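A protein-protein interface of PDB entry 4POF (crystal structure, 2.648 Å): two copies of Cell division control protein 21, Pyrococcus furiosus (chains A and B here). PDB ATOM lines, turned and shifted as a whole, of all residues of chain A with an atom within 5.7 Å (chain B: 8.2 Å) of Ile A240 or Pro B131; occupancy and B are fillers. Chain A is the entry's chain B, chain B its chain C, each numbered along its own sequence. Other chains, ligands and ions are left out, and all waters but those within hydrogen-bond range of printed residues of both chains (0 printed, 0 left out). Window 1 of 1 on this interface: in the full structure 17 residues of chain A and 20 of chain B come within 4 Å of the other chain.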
ATOM      1  N   GLY A 109      31.794  -5.384 -20.569  1.00  0.00           N
ATOM      2  CA  GLY A 109      30.995  -4.297 -20.049  1.00  0.00           C
ATOM      3  C   GLY A 109      29.699  -4.720 -19.413  1.00  0.00           C
ATOM      4  O   GLY A 109      29.446  -5.903 -19.222  1.00  0.00           O
ATOM      5  N   ALA A 110      28.873  -3.731 -19.096  1.00  0.00           N
ATOM      6  CA  ALA A 110      27.628  -3.936 -18.372  1.00  0.00           C
ATOM      7  C   ALA A 110      26.750  -5.009 -19.007  1.00  0.00           C
ATOM      8  O   ALA A 110      25.890  -5.582 -18.338  1.00  0.00           O
ATOM      9  CB  ALA A 110      26.857  -2.603 -18.262  1.00  0.00           C
ATOM     10  N   ILE A 113      27.314  -8.726 -17.280  1.00  0.00           N
ATOM     11  CA  ILE A 113      26.971  -9.009 -15.889  1.00  0.00           C
ATOM     12  C   ILE A 113      26.126 -10.266 -15.796  1.00  0.00           C
ATOM     13  O   ILE A 113      25.077 -10.363 -16.436  1.00  0.00           O
ATOM     14  CB  ILE A 113      26.239  -7.829 -15.241  1.00  0.00           C
ATOM     15  CG1 ILE A 113      27.198  -6.633 -15.171  1.00  0.00           C
ATOM     16  CG2 ILE A 113      25.713  -8.212 -13.874  1.00  0.00           C
ATOM     17  CD1 ILE A 113      26.536  -5.258 -15.119  1.00  0.00           C
ATOM     18  N   VAL A 230      29.548  -8.214 -10.584  1.00  0.00           N
ATOM     19  CA  VAL A 230      29.698  -6.819 -10.157  1.00  0.00           C
ATOM     20  C   VAL A 230      29.552  -6.687  -8.667  1.00  0.00           C
ATOM     21  O   VAL A 230      28.799  -7.423  -8.046  1.00  0.00           O
ATOM     22  CB  VAL A 230      28.676  -5.893 -10.809  1.00  0.00           C
ATOM     23  CG1 VAL A 230      28.911  -5.845 -12.298  1.00  0.00           C
ATOM     24  CG2 VAL A 230      27.251  -6.335 -10.478  1.00  0.00           C
ATOM     25  N   VAL A 231      30.271  -5.734  -8.090  1.00  0.00           N
ATOM     26  CA  VAL A 231      30.122  -5.438  -6.676  1.00  0.00           C
ATOM     27  C   VAL A 231      30.480  -3.976  -6.448  1.00  0.00           C
ATOM     28  O   VAL A 231      31.410  -3.475  -7.074  1.00  0.00           O
ATOM     29  CB  VAL A 231      30.947  -6.426  -5.821  1.00  0.00           C
ATOM     30  CG1 VAL A 231      32.450  -6.162  -5.953  1.00  0.00           C
ATOM     31  CG2 VAL A 231      30.454  -6.402  -4.368  1.00  0.00           C
ATOM     32  N   LEU A 232      29.725  -3.299  -5.579  1.00  0.00           N
ATOM     33  CA  LEU A 232      29.830  -1.839  -5.393  1.00  0.00           C
ATOM     34  C   LEU A 232      31.216  -1.429  -4.939  1.00  0.00           C
ATOM     35  O   LEU A 232      31.900  -2.209  -4.293  1.00  0.00           O
ATOM     36  CB  LEU A 232      28.804  -1.330  -4.378  1.00  0.00           C
ATOM     37  CG  LEU A 232      27.328  -1.713  -4.487  1.00  0.00           C
ATOM     38  CD1 LEU A 232      27.058  -3.149  -3.961  1.00  0.00           C
ATOM     39  CD2 LEU A 232      26.501  -0.712  -3.728  1.00  0.00           C
ATOM     40  N   GLU A 233      31.620  -0.205  -5.262  1.00  0.00           N
ATOM     41  CA  GLU A 233      32.964   0.272  -4.930  1.00  0.00           C
ATOM     42  C   GLU A 233      33.129   0.682  -3.470  1.00  0.00           C
ATOM     43  O   GLU A 233      32.237   1.303  -2.877  1.00  0.00           O
ATOM     44  CB  GLU A 233      33.352   1.440  -5.815  1.00  0.00           C
ATOM     45  CG  GLU A 233      33.438   1.107  -7.274  1.00  0.00           C
ATOM     46  CD  GLU A 233      34.038   2.243  -8.070  1.00  0.00           C
ATOM     47  OE1 GLU A 233      33.585   3.404  -7.917  1.00  0.00           O
ATOM     48  OE2 GLU A 233      34.975   1.973  -8.849  1.00  0.00           O
ATOM     49  N   THR A 238      28.019   4.782  -3.796  1.00  0.00           N
ATOM     50  CA  THR A 238      27.914   5.273  -5.179  1.00  0.00           C
ATOM     51  C   THR A 238      27.298   4.179  -6.046  1.00  0.00           C
ATOM     52  O   THR A 238      27.625   3.011  -5.868  1.00  0.00           O
ATOM     53  CB  THR A 238      29.298   5.661  -5.762  1.00  0.00           C
ATOM     54  OG1 THR A 238      30.150   6.126  -4.711  1.00  0.00           O
ATOM     55  CG2 THR A 238      29.164   6.766  -6.812  1.00  0.00           C
ATOM     56  N   PRO A 239      26.409   4.548  -6.988  1.00  0.00           N
ATOM     57  CA  PRO A 239      25.739   3.527  -7.781  1.00  0.00           C
ATOM     58  C   PRO A 239      26.647   2.987  -8.876  1.00  0.00           C
ATOM     59  O   PRO A 239      26.173   2.523  -9.907  1.00  0.00           O
ATOM     60  CB  PRO A 239      24.553   4.285  -8.368  1.00  0.00           C
ATOM     61  CG  PRO A 239      25.056   5.671  -8.508  1.00  0.00           C
ATOM     62  CD  PRO A 239      25.952   5.903  -7.345  1.00  0.00           C
ATOM     63  N   ILE A 240      27.946   3.046  -8.637  1.00  0.00           N
ATOM     64  CA  ILE A 240      28.940   2.574  -9.594  1.00  0.00           C
ATOM     65  C   ILE A 240      29.565   1.268  -9.083  1.00  0.00           C
ATOM     66  O   ILE A 240      29.655   1.054  -7.875  1.00  0.00           O
ATOM     67  CB  ILE A 240      30.006   3.663  -9.865  1.00  0.00           C
ATOM     68  CG1 ILE A 240      29.434   4.766 -10.760  1.00  0.00           C
ATOM     69  CG2 ILE A 240      31.213   3.093 -10.554  1.00  0.00           C
ATOM     70  CD1 ILE A 240      28.690   5.867 -10.026  1.00  0.00           C
ATOM     71  N   PHE A 241      29.977   0.384  -9.988  1.00  0.00           N
ATOM     72  CA  PHE A 241      30.385  -0.955  -9.571  1.00  0.00           C
ATOM     73  C   PHE A 241      31.763  -1.364 -10.033  1.00  0.00           C
ATOM     74  O   PHE A 241      32.315  -0.804 -10.970  1.00  0.00           O
ATOM     75  CB  PHE A 241      29.362  -1.997 -10.007  1.00  0.00           C
ATOM     76  CG  PHE A 241      28.088  -1.947  -9.235  1.00  0.00           C
ATOM     77  CD1 PHE A 241      27.648  -3.057  -8.545  1.00  0.00           C
ATOM     78  CD2 PHE A 241      27.323  -0.800  -9.201  1.00  0.00           C
ATOM     79  CE1 PHE A 241      26.457  -3.021  -7.832  1.00  0.00           C
ATOM     80  CE2 PHE A 241      26.159  -0.758  -8.490  1.00  0.00           C
ATOM     81  CZ  PHE A 241      25.719  -1.869  -7.804  1.00  0.00           C
ATOM     82  N   ARG A 242      32.306  -2.352  -9.341  1.00  0.00           N
ATOM     83  CA  ARG A 242      33.613  -2.884  -9.624  1.00  0.00           C
ATOM     84  C   ARG A 242      33.344  -4.239 -10.235  1.00  0.00           C
ATOM     85  O   ARG A 242      32.476  -4.973  -9.752  1.00  0.00           O
ATOM     86  CB  ARG A 242      34.398  -2.993  -8.316  1.00  0.00           C
ATOM     87  CG  ARG A 242      35.556  -3.983  -8.279  1.00  0.00           C
ATOM     88  CD  ARG A 242      36.204  -3.986  -6.881  1.00  0.00           C
ATOM     89  NE  ARG A 242      37.133  -5.102  -6.647  1.00  0.00           N
ATOM     90  CZ  ARG A 242      38.239  -5.353  -7.357  1.00  0.00           C
ATOM     91  NH1 ARG A 242      39.009  -6.384  -7.033  1.00  0.00           N
ATOM     92  NH2 ARG A 242      38.577  -4.594  -8.396  1.00  0.00           N
ATOM     93  N   LYS A 243      34.061  -4.565 -11.310  1.00  0.00           N
ATOM     94  CA  LYS A 243      33.801  -5.827 -12.004  1.00  0.00           C
ATOM     95  C   LYS A 243      34.904  -6.872 -11.870  1.00  0.00           C
ATOM     96  O   LYS A 243      36.093  -6.589 -12.065  1.00  0.00           O
ATOM     97  CB  LYS A 243      33.365  -5.616 -13.466  1.00  0.00           C
ATOM     98  CG  LYS A 243      34.288  -4.803 -14.330  1.00  0.00           C
ATOM     99  CD  LYS A 243      33.540  -4.288 -15.531  1.00  0.00           C
ATOM    100  CE  LYS A 243      34.493  -3.981 -16.683  1.00  0.00           C
ATOM    101  NZ  LYS A 243      35.804  -3.349 -16.306  1.00  0.00           N
ATOM    102  N   GLU B 128      37.931   4.994 -16.380  1.00  0.00           N
ATOM    103  CA  GLU B 128      37.768   3.649 -16.912  1.00  0.00           C
ATOM    104  C   GLU B 128      36.288   3.357 -16.878  1.00  0.00           C
ATOM    105  O   GLU B 128      35.555   3.991 -16.130  1.00  0.00           O
ATOM    106  CB  GLU B 128      38.560   2.621 -16.103  1.00  0.00           C
ATOM    107  CG  GLU B 128      38.262   2.598 -14.601  1.00  0.00           C
ATOM    108  CD  GLU B 128      38.679   1.296 -13.909  1.00  0.00           C
ATOM    109  OE1 GLU B 128      38.622   1.251 -12.662  1.00  0.00           O
ATOM    110  OE2 GLU B 128      39.049   0.319 -14.601  1.00  0.00           O
ATOM    111  N   ILE B 129      35.839   2.410 -17.686  1.00  0.00           N
ATOM    112  CA  ILE B 129      34.407   2.249 -17.879  1.00  0.00           C
ATOM    113  C   ILE B 129      33.776   1.254 -16.919  1.00  0.00           C
ATOM    114  O   ILE B 129      33.977   0.049 -17.020  1.00  0.00           O
ATOM    115  CB  ILE B 129      34.088   1.909 -19.333  1.00  0.00           C
ATOM    116  CG1 ILE B 129      34.653   3.008 -20.236  1.00  0.00           C
ATOM    117  CG2 ILE B 129      32.567   1.695 -19.515  1.00  0.00           C
ATOM    118  CD1 ILE B 129      34.779   2.618 -21.659  1.00  0.00           C
ATOM    119  N   LYS B 130      32.989   1.773 -15.997  1.00  0.00           N
ATOM    120  CA  LYS B 130      32.388   0.951 -14.966  1.00  0.00           C
ATOM    121  C   LYS B 130      30.882   0.808 -15.165  1.00  0.00           C
ATOM    122  O   LYS B 130      30.260   1.642 -15.812  1.00  0.00           O
ATOM    123  CB  LYS B 130      32.695   1.570 -13.611  1.00  0.00           C
ATOM    124  CG  LYS B 130      34.166   1.919 -13.428  1.00  0.00           C
ATOM    125  CD  LYS B 130      34.403   2.846 -12.248  1.00  0.00           C
ATOM    126  CE  LYS B 130      35.890   2.951 -11.965  1.00  0.00           C
ATOM    127  NZ  LYS B 130      36.247   4.041 -11.024  1.00  0.00           N
ATOM    128  N   PRO B 131      30.291  -0.264 -14.628  1.00  0.00           N
ATOM    129  CA  PRO B 131      28.838  -0.420 -14.657  1.00  0.00           C
ATOM    130  C   PRO B 131      28.152   0.510 -13.679  1.00  0.00           C
ATOM    131  O   PRO B 131      28.632   0.690 -12.577  1.00  0.00           O
ATOM    132  CB  PRO B 131      28.638  -1.864 -14.206  1.00  0.00           C
ATOM    133  CG  PRO B 131      29.912  -2.524 -14.555  1.00  0.00           C
ATOM    134  CD  PRO B 131      30.962  -1.515 -14.264  1.00  0.00           C
ATOM    135  N   PHE B 132      27.034   1.085 -14.086  1.00  0.00           N
ATOM    136  CA  PHE B 132      26.182   1.883 -13.204  1.00  0.00           C
ATOM    137  C   PHE B 132      24.780   1.263 -13.090  1.00  0.00           C
ATOM    138  O   PHE B 132      24.237   0.803 -14.100  1.00  0.00           O
ATOM    139  CB  PHE B 132      26.114   3.294 -13.790  1.00  0.00           C
ATOM    140  CG  PHE B 132      24.924   4.114 -13.349  1.00  0.00           C
ATOM    141  CD1 PHE B 132      24.776   4.518 -12.033  1.00  0.00           C
ATOM    142  CD2 PHE B 132      23.982   4.540 -14.285  1.00  0.00           C
ATOM    143  CE1 PHE B 132      23.692   5.312 -11.650  1.00  0.00           C
ATOM    144  CE2 PHE B 132      22.894   5.333 -13.903  1.00  0.00           C
ATOM    145  CZ  PHE B 132      22.750   5.718 -12.585  1.00  0.00           C
ATOM    146  N   VAL B 133      24.185   1.240 -11.891  1.00  0.00           N
ATOM    147  CA  VAL B 133      22.782   0.771 -11.756  1.00  0.00           C
ATOM    148  C   VAL B 133      21.824   1.868 -12.130  1.00  0.00           C
ATOM    149  O   VAL B 133      21.529   2.723 -11.290  1.00  0.00           O
ATOM    150  CB  VAL B 133      22.322   0.473 -10.317  1.00  0.00           C
ATOM    151  CG1 VAL B 133      21.468  -0.776 -10.303  1.00  0.00           C
ATOM    152  CG2 VAL B 133      23.450   0.374  -9.359  1.00  0.00           C
ATOM    153  N   SER B 134      21.308   1.862 -13.353  1.00  0.00           N
ATOM    154  CA  SER B 134      20.388   2.925 -13.718  1.00  0.00           C
ATOM    155  C   SER B 134      19.076   2.725 -12.963  1.00  0.00           C
ATOM    156  O   SER B 134      18.442   3.679 -12.540  1.00  0.00           O
ATOM    157  CB  SER B 134      20.206   3.021 -15.229  1.00  0.00           C
ATOM    158  OG  SER B 134      19.800   1.787 -15.774  1.00  0.00           O
ATOM    159  N   GLN B 151      18.154   5.251 -10.109  1.00  0.00           N
ATOM    160  CA  GLN B 151      19.338   5.923  -9.555  1.00  0.00           C
ATOM    161  C   GLN B 151      19.810   7.027 -10.465  1.00  0.00           C
ATOM    162  O   GLN B 151      19.366   7.128 -11.602  1.00  0.00           O
ATOM    163  CB  GLN B 151      20.498   4.945  -9.330  1.00  0.00           C
ATOM    164  CG  GLN B 151      20.162   3.748  -8.490  1.00  0.00           C
ATOM    165  CD  GLN B 151      19.841   4.104  -7.067  1.00  0.00           C
ATOM    166  OE1 GLN B 151      20.643   4.725  -6.371  1.00  0.00           O
ATOM    167  NE2 GLN B 151      18.663   3.705  -6.618  1.00  0.00           N
ATOM    168  N   LYS B 152      20.726   7.840  -9.948  1.00  0.00           N
ATOM    169  CA  LYS B 152      21.284   8.970 -10.675  1.00  0.00           C
ATOM    170  C   LYS B 152      22.799   8.843 -10.635  1.00  0.00           C
ATOM    171  O   LYS B 152      23.373   8.691  -9.572  1.00  0.00           O
ATOM    172  CB  LYS B 152      20.839  10.270 -10.011  1.00  0.00           C
ATOM    173  CG  LYS B 152      20.241  11.298 -10.946  1.00  0.00           C
ATOM    174  CD  LYS B 152      18.818  10.949 -11.352  1.00  0.00           C
ATOM    175  CE  LYS B 152      18.071  12.168 -11.891  1.00  0.00           C
ATOM    176  NZ  LYS B 152      17.588  13.067 -10.794  1.00  0.00           N
ATOM    177  N   PRO B 153      23.458   8.905 -11.791  1.00  0.00           N
ATOM    178  CA  PRO B 153      24.889   8.633 -11.900  1.00  0.00           C
ATOM    179  C   PRO B 153      25.798   9.581 -11.111  1.00  0.00           C
ATOM    180  O   PRO B 153      26.906   9.183 -10.736  1.00  0.00           O
ATOM    181  CB  PRO B 153      25.157   8.778 -13.392  1.00  0.00           C
ATOM    182  CG  PRO B 153      24.086   9.672 -13.882  1.00  0.00           C
ATOM    183  CD  PRO B 153      22.884   9.345 -13.071  1.00  0.00           C
ATOM    184  N   TYR B 154      25.334  10.806 -10.858  1.00  0.00           N
ATOM    185  CA  TYR B 154      26.112  11.819 -10.124  1.00  0.00           C
ATOM    186  C   TYR B 154      25.811  11.849  -8.617  1.00  0.00           C
ATOM    187  O   TYR B 154      26.615  12.349  -7.818  1.00  0.00           O
ATOM    188  CB  TYR B 154      25.901  13.209 -10.733  1.00  0.00           C
ATOM    189  CG  TYR B 154      24.463  13.662 -10.750  1.00  0.00           C
ATOM    190  CD1 TYR B 154      23.903  14.310  -9.650  1.00  0.00           C
ATOM    191  CD2 TYR B 154      23.661  13.451 -11.866  1.00  0.00           C
ATOM    192  CE1 TYR B 154      22.573  14.728  -9.657  1.00  0.00           C
ATOM    193  CE2 TYR B 154      22.333  13.870 -11.891  1.00  0.00           C
ATOM    194  CZ  TYR B 154      21.796  14.506 -10.777  1.00  0.00           C
ATOM    195  OH  TYR B 154      20.488  14.930 -10.775  1.00  0.00           O
ATOM    196  N   GLU B 155      24.642  11.339  -8.243  1.00  0.00           N
ATOM    197  CA  GLU B 155      24.268  11.206  -6.851  1.00  0.00           C
ATOM    198  C   GLU B 155      24.857   9.917  -6.286  1.00  0.00           C
ATOM    199  O   GLU B 155      25.504   9.140  -6.998  1.00  0.00           O
ATOM    200  CB  GLU B 155      22.745  11.189  -6.696  1.00  0.00           C
ATOM    201  CG  GLU B 155      22.075  12.559  -6.662  1.00  0.00           C
ATOM    202  CD  GLU B 155      20.554  12.470  -6.488  1.00  0.00           C
ATOM    203  OE1 GLU B 155      20.078  11.616  -5.706  1.00  0.00           O
ATOM    204  OE2 GLU B 155      19.827  13.260  -7.130  1.00  0.00           O
ATOM    205  N   SER B 156      24.634   9.714  -4.993  1.00  0.00           N
ATOM    206  CA  SER B 156      25.033   8.505  -4.315  1.00  0.00           C
ATOM    207  C   SER B 156      23.923   7.468  -4.461  1.00  0.00           C
ATOM    208  O   SER B 156      22.835   7.785  -4.947  1.00  0.00           O
ATOM    209  CB  SER B 156      25.279   8.809  -2.847  1.00  0.00           C
ATOM    210  OG  SER B 156      24.082   9.257  -2.256  1.00  0.00           O
ATOM    211  N   LEU B 157      24.207   6.234  -4.047  1.00  0.00           N
ATOM    212  CA  LEU B 157      23.258   5.137  -4.158  1.00  0.00           C
ATOM    213  C   LEU B 157      22.159   5.270  -3.123  1.00  0.00           C
ATOM    214  O   LEU B 157      22.428   5.404  -1.933  1.00  0.00           O
ATOM    215  CB  LEU B 157      23.959   3.787  -4.008  1.00  0.00           C
ATOM    216  CG  LEU B 157      22.997   2.605  -3.874  1.00  0.00           C
ATOM    217  CD1 LEU B 157      22.424   2.194  -5.219  1.00  0.00           C
ATOM    218  CD2 LEU B 157      23.662   1.431  -3.196  1.00  0.00           C
ATOM    219  N   SER B 179      18.937  -2.990 -13.375  1.00  0.00           N
ATOM    220  CA  SER B 179      19.346  -2.545 -14.698  1.00  0.00           C
ATOM    221  C   SER B 179      20.672  -1.795 -14.665  1.00  0.00           C
ATOM    222  O   SER B 179      20.809  -0.780 -13.971  1.00  0.00           O
ATOM    223  CB  SER B 179      18.256  -1.672 -15.310  1.00  0.00           C
ATOM    224  OG  SER B 179      17.107  -2.440 -15.608  1.00  0.00           O
ATOM    225  N   PHE B 180      21.646  -2.296 -15.416  1.00  0.00           N
ATOM    226  CA  PHE B 180      22.966  -1.681 -15.455  1.00  0.00           C
ATOM    227  C   PHE B 180      23.246  -1.106 -16.820  1.00  0.00           C
ATOM    228  O   PHE B 180      22.813  -1.652 -17.840  1.00  0.00           O
ATOM    229  CB  PHE B 180      24.054  -2.706 -15.136  1.00  0.00           C
ATOM    230  CG  PHE B 180      23.988  -3.253 -13.746  1.00  0.00           C
ATOM    231  CD1 PHE B 180      24.987  -2.975 -12.834  1.00  0.00           C
ATOM    232  CD2 PHE B 180      22.929  -4.051 -13.349  1.00  0.00           C
ATOM    233  CE1 PHE B 180      24.917  -3.482 -11.549  1.00  0.00           C
ATOM    234  CE2 PHE B 180      22.858  -4.557 -12.064  1.00  0.00           C
ATOM    235  CZ  PHE B 180      23.852  -4.277 -11.167  1.00  0.00           C
ATOM    236  N   VAL B 181      23.983  -0.006 -16.848  1.00  0.00           N
ATOM    237  CA  VAL B 181      24.508   0.507 -18.106  1.00  0.00           C
ATOM    238  C   VAL B 181      25.942   0.923 -17.872  1.00  0.00           C
ATOM    239  O   VAL B 181      26.317   1.203 -16.737  1.00  0.00           O
ATOM    240  CB  VAL B 181      23.677   1.705 -18.644  1.00  0.00           C
ATOM    241  CG1 VAL B 181      22.287   1.258 -19.107  1.00  0.00           C
ATOM    242  CG2 VAL B 181      23.583   2.807 -17.608  1.00  0.00           C
ATOM    243  N   ASN B 182      26.741   0.970 -18.936  1.00  0.00           N
ATOM    244  CA  ASN B 182      28.112   1.491 -18.823  1.00  0.00           C
ATOM    245  C   ASN B 182      28.158   2.963 -18.418  1.00  0.00           C
ATOM    246  O   ASN B 182      27.288   3.739 -18.808  1.00  0.00           O
ATOM    247  CB  ASN B 182      28.886   1.266 -20.111  1.00  0.00           C
ATOM    248  CG  ASN B 182      29.001  -0.199 -20.469  1.00  0.00           C
ATOM    249  OD1 ASN B 182      29.380  -1.030 -19.643  1.00  0.00           O
ATOM    250  ND2 ASN B 182      28.679  -0.524 -21.709  1.00  0.00           N
ATOM    251  N   PHE B 183      29.167   3.319 -17.622  1.00  0.00           N
ATOM    252  CA  PHE B 183      29.370   4.667 -17.054  1.00  0.00           C
ATOM    253  C   PHE B 183      30.819   5.078 -17.295  1.00  0.00           C
ATOM    254  O   PHE B 183      31.718   4.249 -17.200  1.00  0.00           O
ATOM    255  CB  PHE B 183      29.082   4.622 -15.547  1.00  0.00           C
ATOM    256  CG  PHE B 183      29.580   5.817 -14.774  1.00  0.00           C
ATOM    257  CD1 PHE B 183      28.686   6.704 -14.181  1.00  0.00           C
ATOM    258  CD2 PHE B 183      30.951   6.034 -14.599  1.00  0.00           C
ATOM    259  CE1 PHE B 183      29.160   7.813 -13.456  1.00  0.00           C
ATOM    260  CE2 PHE B 183      31.438   7.141 -13.884  1.00  0.00           C
ATOM    261  CZ  PHE B 183      30.544   8.028 -13.313  1.00  0.00           C
ATOM    262  N   GLN B 184      31.069   6.343 -17.603  1.00  0.00           N
ATOM    263  CA  GLN B 184      32.446   6.793 -17.778  1.00  0.00           C
ATOM    264  C   GLN B 184      32.638   8.272 -17.500  1.00  0.00           C
ATOM    265  O   GLN B 184      32.043   9.113 -18.148  1.00  0.00           O
ATOM    266  CB  GLN B 184      32.977   6.469 -19.170  1.00  0.00           C
ATOM    267  CG  GLN B 184      34.406   6.924 -19.356  1.00  0.00           C
ATOM    268  CD  GLN B 184      34.885   6.823 -20.772  1.00  0.00           C
ATOM    269  OE1 GLN B 184      34.110   6.972 -21.711  1.00  0.00           O
ATOM    270  NE2 GLN B 184      36.179   6.594 -20.943  1.00  0.00           N
ATOM    271  N   SER B 185      33.498   8.580 -16.544  1.00  0.00           N
ATOM    272  CA  SER B 185      33.841   9.960 -16.231  1.00  0.00           C
ATOM    273  C   SER B 185      34.875  10.506 -17.200  1.00  0.00           C
ATOM    274  O   SER B 185      35.633   9.754 -17.818  1.00  0.00           O
ATOM    275  CB  SER B 185      34.382  10.069 -14.803  1.00  0.00           C
ATOM    276  OG  SER B 185      35.610   9.367 -14.671  1.00  0.00           O
ATOM    277  N   ILE B 207      30.069  13.299 -16.833  1.00  0.00           N
ATOM    278  CA  ILE B 207      29.807  11.873 -16.941  1.00  0.00           C
ATOM    279  C   ILE B 207      29.056  11.444 -18.228  1.00  0.00           C
ATOM    280  O   ILE B 207      28.277  12.213 -18.806  1.00  0.00           O
ATOM    281  CB  ILE B 207      29.171  11.327 -15.636  1.00  0.00           C
ATOM    282  CG1 ILE B 207      27.648  11.448 -15.611  1.00  0.00           C
ATOM    283  CG2 ILE B 207      29.763  12.045 -14.411  1.00  0.00           C
ATOM    284  CD1 ILE B 207      27.131  11.468 -14.187  1.00  0.00           C
ATOM    285  N   LEU B 209      26.928   8.104 -20.111  1.00  0.00           N
ATOM    286  CA  LEU B 209      26.247   6.840 -19.876  1.00  0.00           C
ATOM    287  C   LEU B 209      25.903   6.082 -21.163  1.00  0.00           C
ATOM    288  O   LEU B 209      25.712   6.676 -22.243  1.00  0.00           O
ATOM    289  CB  LEU B 209      24.968   7.033 -19.059  1.00  0.00           C
ATOM    290  CG  LEU B 209      25.026   7.660 -17.682  1.00  0.00           C
ATOM    291  CD1 LEU B 209      23.757   7.277 -16.978  1.00  0.00           C
ATOM    292  CD2 LEU B 209      26.189   7.170 -16.897  1.00  0.00           C
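OD1 of Asn B182 lies within hydrogen-bond range of N of Ala A110, 2.8 Å away.
The side-chain carboxylate (OE2) of Glu A233 is in salt-bridge range of the side-chain amino group (NZ) of Lys B130 (3.3 Å).
The backbone carbonyl oxygen of Pro A239 sits at hydrogen-bond distance from the backbone NH of Val B133, at 3.1 Å.
The backbone carbonyl oxygen of Pro B131 is in hydrogen-bond range of the backbone NH of Phe A241.
The backbone NH of Phe B183 is in hydrogen-bond range of the backbone carbonyl oxygen of Lys B130, 2.7 Å away.
N of Phe B132 lies within hydrogen-bond range of O of Val B181, 2.7 Å away.
The side-chain amino group of Lys B152 sits at hydrogen-bond distance from the side-chain hydroxyl of Tyr B154 (3.4 Å).
Gly A109 touches Asn B182.
Leu B157 touches Leu A232.
Pro A239 touches Phe B132.
Pro A239 touches Lys B152 (CG to O, 3.6 Å).
CD of Pro A239 touches C of Ser B156 (3.9 Å).
CD of Pro A239 touches N of Leu B157, at 3.7 Å.
Lys B130 touches Ile A240 (CD to CG2, 3.6 Å).
Ile A240 touches Phe B183.
Phe A241 touches Lys B130 (O to CB, 3.6 Å).
Lys A243 touches Ile B129 (NZ to O, 3.9 Å).
Printed residues of chain B within 4 Å of Gly A109: Asn B182 (3.7 Å).
Pro A239 touches just these residues of chain B: Phe B132 (3.2 Å), Val B133 (3.1 Å), Lys B152 (3.6 Å), Glu B155 (3.3 Å), Ser B156 (3.9 Å) and Leu B157 (3.7 Å).
Of chain B, only Lys B130 (3.6 Å), Pro B131 (3.5 Å), Pro B153 (3.8 Å) and Phe B183 (3.97 Å) come within 4 Å of Ile A240.
Of the printed residues of chain A, Lys B130 touches Glu A233, Ile A240 and Phe A241.
Printed residues of chain A within 4 Å of Pro B131: Ile A240 (3.5 Å), Phe A241 (2.9 Å) and Lys A243 (3.99 Å).
Of the printed residues of chain A, Glu B155 touches Pro A239.
The nearest printed residue of chain B that does not touch Phe A241 is Phe B180 (4.05 Å).
Of the 23 printed residues of chain B, 14 touch a printed residue of chain A.
Printed residues of chain B that touch a printed residue of chain A: Ile B129, Lys B130, Pro B131, Phe B132, Val B133, Lys B152, Pro B153, Glu B155, Ser B156, Leu B157, Phe B180, Val B181, Asn B182 and Phe B183.
Of the 13 printed residues of chain A, 11 touch a printed residue of chain B.
Printed residues of chain A that touch a printed residue of chain B: Gly A109, Ala A110, Ile A113, Val A230, Leu A232, Glu A233, Thr A238, Pro A239, Ile A240, Phe A241 and Lys A243.
Hydrophobic or aromatic side chains of chain A that line the printed part of chain B: Ala A110, Ile A113, Val A230, Leu A232, Pro A239, Ile A240 and Phe A241.
Along chain A the printed residues that touch a printed residue of chain B span positions 109 to 243.
No position is printed for both chains.
Of the 23 pairs that touch across the chains among the printed residues, none has its exchanged pair printed and touching as well.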
